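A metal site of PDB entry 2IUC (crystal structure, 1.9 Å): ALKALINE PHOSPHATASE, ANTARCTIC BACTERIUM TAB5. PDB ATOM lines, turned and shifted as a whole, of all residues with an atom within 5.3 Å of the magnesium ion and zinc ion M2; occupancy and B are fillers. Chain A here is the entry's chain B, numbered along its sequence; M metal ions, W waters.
The side-chain carboxylate (OE1) of Glu 254 lies within hydrogen-bond range of the side-chain hydroxyl (OG) of Ser 256, at 2.6 Å.
The backbone carbonyl oxygen (O) of Asp 43 is in hydrogen-bond range of the backbone NH (N) of Asp 259, 3.0 Å away.
A ring nitrogen (NE2) of His 302 sits close to a ring nitrogen (ND1) of His 337.
The backbone NH (N) of Gly 44 lies close to the backbone carbonyl oxygen (O) of His 302, at 3.1 Å.
The side-chain carboxylate (OD1) of Asp 301 sits at hydrogen-bond distance from the backbone NH (N) of Gly 44 (3.1 Å).
His 135 touches the magnesium ion (ND1 to MG, 3.998 Å).
Of the 15 residues printed, 4 come within 4 Å of the magnesium ion.
The nearest printed residue that does not touch the magnesium ion is Ser 84 (4.5 Å).
OE2 of Glu 254 is bound to the magnesium ion, at 1.9 Å.
Water W2 binds the magnesium ion (2.2 Å).
Water W3 is bound to the magnesium ion.
The magnesium ion is bound by OD2 of Asp 43 (2.2 Å).
The magnesium ion is bound by the side-chain hydroxyl (OG1) of Thr 137, 2.3 Å away.
Water W1 binds the magnesium ion, 2.3 Å away.
Zinc ion M2 is bound by OD1 of Asp 43 (1.9 Å), NE2 of His 302 (2.0 Å), OD2 of Asp 301 (2.1 Å) and OG of Ser 84 (2.1 Å).
Zinc ion M2 has four donor atoms within binding distance.
Slightly farther from zinc ion M2 lies OD2 of Asp 43 (2.8 Å).
Water W3 lies within hydrogen-bond range of ND1 of His 135 (2.7 Å), OE1 of Glu 254 (2.9 Å) and OG of Ser 131 (3.4 Å).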
ATOM      1  N   ASP A  43     -27.334  -7.425   0.292  1.00  0.00           N
ATOM      2  CA  ASP A  43     -26.450  -6.692  -0.593  1.00  0.00           C
ATOM      3  C   ASP A  43     -24.992  -6.970  -0.229  1.00  0.00           C
ATOM      4  O   ASP A  43     -24.643  -6.822   0.906  1.00  0.00           O
ATOM      5  CB  ASP A  43     -26.736  -5.193  -0.413  1.00  0.00           C
ATOM      6  CG  ASP A  43     -26.211  -4.310  -1.593  1.00  0.00           C
ATOM      7  OD1 ASP A  43     -24.991  -4.305  -1.843  1.00  0.00           O
ATOM      8  OD2 ASP A  43     -26.997  -3.547  -2.173  1.00  0.00           O
ATOM      9  N   GLY A  44     -24.121  -7.343  -1.175  1.00  0.00           N
ATOM     10  CA  GLY A  44     -22.710  -7.428  -0.782  1.00  0.00           C
ATOM     11  C   GLY A  44     -22.373  -8.801  -0.212  1.00  0.00           C
ATOM     12  O   GLY A  44     -21.254  -9.012   0.193  1.00  0.00           O
ATOM     13  N   ASP A  83     -22.178  -2.776  -9.776  1.00  0.00           N
ATOM     14  CA  ASP A  83     -22.668  -2.061  -8.543  1.00  0.00           C
ATOM     15  C   ASP A  83     -24.076  -2.525  -8.156  1.00  0.00           C
ATOM     16  O   ASP A  83     -24.703  -3.340  -8.873  1.00  0.00           O
ATOM     17  CB  ASP A  83     -22.525  -0.543  -8.680  1.00  0.00           C
ATOM     18  CG  ASP A  83     -23.715   0.145  -9.463  1.00  0.00           C
ATOM     19  OD1 ASP A  83     -24.406  -0.467 -10.318  1.00  0.00           O
ATOM     20  OD2 ASP A  83     -23.957   1.345  -9.210  1.00  0.00           O
ATOM     21  N   SER A  84     -24.609  -1.994  -7.067  1.00  0.00           N
ATOM     22  CA  SER A  84     -25.956  -2.345  -6.602  1.00  0.00           C
ATOM     23  C   SER A  84     -27.079  -1.974  -7.550  1.00  0.00           C
ATOM     24  O   SER A  84     -28.110  -2.642  -7.603  1.00  0.00           O
ATOM     25  CB  SER A  84     -26.212  -1.641  -5.304  1.00  0.00           C
ATOM     26  OG  SER A  84     -25.143  -1.968  -4.416  1.00  0.00           O
ATOM     27  N   SER A 131     -31.278   0.465   4.563  1.00  0.00           N
ATOM     28  CA  SER A 131     -30.742   1.736   4.079  1.00  0.00           C
ATOM     29  C   SER A 131     -31.871   2.772   3.960  1.00  0.00           C
ATOM     30  O   SER A 131     -33.038   2.493   4.308  1.00  0.00           O
ATOM     31  CB  SER A 131     -30.118   1.526   2.662  1.00  0.00           C
ATOM     32  OG  SER A 131     -31.121   1.077   1.727  1.00  0.00           O
ATOM     33  N   HIS A 135     -32.116   4.365  -1.717  1.00  0.00           N
ATOM     34  CA  HIS A 135     -30.788   3.766  -1.990  1.00  0.00           C
ATOM     35  C   HIS A 135     -30.910   2.739  -3.111  1.00  0.00           C
ATOM     36  O   HIS A 135     -32.014   2.375  -3.477  1.00  0.00           O
ATOM     37  CB  HIS A 135     -30.196   3.212  -0.709  1.00  0.00           C
ATOM     38  CG  HIS A 135     -28.711   3.059  -0.768  1.00  0.00           C
ATOM     39  ND1 HIS A 135     -28.111   1.881  -1.149  1.00  0.00           N
ATOM     40  CD2 HIS A 135     -27.705   3.900  -0.407  1.00  0.00           C
ATOM     41  CE1 HIS A 135     -26.798   2.017  -1.064  1.00  0.00           C
ATOM     42  NE2 HIS A 135     -26.514   3.248  -0.650  1.00  0.00           N
ATOM     43  N   ALA A 136     -29.803   2.350  -3.782  1.00  0.00           N
ATOM     44  CA  ALA A 136     -29.967   1.816  -5.159  1.00  0.00           C
ATOM     45  C   ALA A 136     -30.833   0.551  -5.291  1.00  0.00           C
ATOM     46  O   ALA A 136     -31.527   0.329  -6.311  1.00  0.00           O
ATOM     47  CB  ALA A 136     -28.548   1.562  -5.865  1.00  0.00           C
ATOM     48  N   THR A 137     -30.741  -0.359  -4.294  1.00  0.00           N
ATOM     49  CA  THR A 137     -31.456  -1.655  -4.362  1.00  0.00           C
ATOM     50  C   THR A 137     -32.975  -1.461  -4.283  1.00  0.00           C
ATOM     51  O   THR A 137     -33.695  -1.816  -5.283  1.00  0.00           O
ATOM     52  CB  THR A 137     -30.921  -2.651  -3.291  1.00  0.00           C
ATOM     53  OG1 THR A 137     -29.502  -2.688  -3.336  1.00  0.00           O
ATOM     54  CG2 THR A 137     -31.511  -4.112  -3.453  1.00  0.00           C
ATOM     55  N   PRO A 138     -33.479  -0.829  -3.167  1.00  0.00           N
ATOM     56  CA  PRO A 138     -34.952  -0.542  -3.116  1.00  0.00           C
ATOM     57  C   PRO A 138     -35.397   0.346  -4.337  1.00  0.00           C
ATOM     58  O   PRO A 138     -36.432   0.065  -4.928  1.00  0.00           O
ATOM     59  CB  PRO A 138     -35.156   0.137  -1.762  1.00  0.00           C
ATOM     60  CG  PRO A 138     -33.740   0.590  -1.278  1.00  0.00           C
ATOM     61  CD  PRO A 138     -32.750  -0.317  -1.970  1.00  0.00           C
ATOM     62  N   GLU A 254     -34.573  -5.991   1.753  1.00  0.00           N
ATOM     63  CA  GLU A 254     -33.143  -5.918   1.568  1.00  0.00           C
ATOM     64  C   GLU A 254     -32.430  -5.814   2.896  1.00  0.00           C
ATOM     65  O   GLU A 254     -32.796  -4.967   3.740  1.00  0.00           O
ATOM     66  CB  GLU A 254     -32.779  -4.709   0.733  1.00  0.00           C
ATOM     67  CG  GLU A 254     -31.308  -4.773   0.315  1.00  0.00           C
ATOM     68  CD  GLU A 254     -30.654  -3.448  -0.057  1.00  0.00           C
ATOM     69  OE1 GLU A 254     -31.223  -2.383   0.245  1.00  0.00           O
ATOM     70  OE2 GLU A 254     -29.508  -3.454  -0.610  1.00  0.00           O
ATOM     71  N   SER A 256     -29.508  -4.330   3.656  1.00  0.00           N
ATOM     72  CA  SER A 256     -28.765  -3.328   2.949  1.00  0.00           C
ATOM     73  C   SER A 256     -27.348  -3.101   3.427  1.00  0.00           C
ATOM     74  O   SER A 256     -26.466  -2.711   2.628  1.00  0.00           O
ATOM     75  CB  SER A 256     -29.513  -1.976   3.027  1.00  0.00           C
ATOM     76  OG  SER A 256     -30.926  -2.145   2.820  1.00  0.00           O
ATOM     77  N   ASP A 259     -23.313  -5.031   2.863  1.00  0.00           N
ATOM     78  CA  ASP A 259     -22.394  -4.340   1.945  1.00  0.00           C
ATOM     79  C   ASP A 259     -21.495  -3.298   2.596  1.00  0.00           C
ATOM     80  O   ASP A 259     -20.311  -3.162   2.301  1.00  0.00           O
ATOM     81  CB  ASP A 259     -23.234  -3.637   0.877  1.00  0.00           C
ATOM     82  CG  ASP A 259     -22.407  -2.915  -0.203  1.00  0.00           C
ATOM     83  OD1 ASP A 259     -21.695  -3.547  -0.942  1.00  0.00           O
ATOM     84  OD2 ASP A 259     -22.517  -1.697  -0.354  1.00  0.00           O
ATOM     85  N   ASP A 301     -26.736  -9.198  -4.764  1.00  0.00           N
ATOM     86  CA  ASP A 301     -26.490  -8.524  -6.004  1.00  0.00           C
ATOM     87  C   ASP A 301     -25.020  -8.731  -6.478  1.00  0.00           C
ATOM     88  O   ASP A 301     -24.757  -8.691  -7.676  1.00  0.00           O
ATOM     89  CB  ASP A 301     -26.874  -7.018  -5.888  1.00  0.00           C
ATOM     90  CG  ASP A 301     -26.178  -6.300  -4.721  1.00  0.00           C
ATOM     91  OD1 ASP A 301     -25.674  -7.016  -3.784  1.00  0.00           O
ATOM     92  OD2 ASP A 301     -26.114  -5.013  -4.773  1.00  0.00           O
ATOM     93  N   HIS A 302     -24.121  -8.926  -5.528  1.00  0.00           N
ATOM     94  CA  HIS A 302     -22.646  -9.070  -5.760  1.00  0.00           C
ATOM     95  C   HIS A 302     -22.061  -9.326  -4.350  1.00  0.00           C
ATOM     96  O   HIS A 302     -22.778  -9.232  -3.299  1.00  0.00           O
ATOM     97  CB  HIS A 302     -22.023  -7.770  -6.373  1.00  0.00           C
ATOM     98  CG  HIS A 302     -22.252  -6.562  -5.495  1.00  0.00           C
ATOM     99  ND1 HIS A 302     -21.495  -6.311  -4.347  1.00  0.00           N
ATOM    100  CD2 HIS A 302     -23.236  -5.624  -5.512  1.00  0.00           C
ATOM    101  CE1 HIS A 302     -22.015  -5.263  -3.710  1.00  0.00           C
ATOM    102  NE2 HIS A 302     -23.048  -4.817  -4.415  1.00  0.00           N
ATOM    103  N   HIS A 337     -16.388  -4.042  -4.574  1.00  0.00           N
ATOM    104  CA  HIS A 337     -17.144  -5.225  -4.900  1.00  0.00           C
ATOM    105  C   HIS A 337     -16.225  -6.246  -5.605  1.00  0.00           C
ATOM    106  O   HIS A 337     -15.134  -5.897  -6.085  1.00  0.00           O
ATOM    107  CB  HIS A 337     -18.353  -4.903  -5.838  1.00  0.00           C
ATOM    108  CG  HIS A 337     -19.314  -3.908  -5.252  1.00  0.00           C
ATOM    109  ND1 HIS A 337     -20.314  -3.323  -6.000  1.00  0.00           N
ATOM    110  CD2 HIS A 337     -19.377  -3.355  -4.020  1.00  0.00           C
ATOM    111  CE1 HIS A 337     -20.980  -2.454  -5.234  1.00  0.00           C
ATOM    112  NE2 HIS A 337     -20.438  -2.485  -4.029  1.00  0.00           N
HETATM  113 MG    MG M   1     -28.459  -2.093  -1.411  1.00  0.00          MG
HETATM  114 ZN    ZN M   2     -24.702  -3.900  -3.725  1.00  0.00          ZN
HETATM  115 ZN    ZN M   3     -21.174  -1.658  -2.269  1.00  0.00          ZN
HETATM  116  O   HOH W   1     -27.378  -0.504  -2.750  1.00  0.00           O
HETATM  117  O   HOH W   2     -27.064  -1.647   0.164  1.00  0.00           O
HETATM  118  O   HOH W   3     -29.632  -0.315  -0.938  1.00  0.00           O
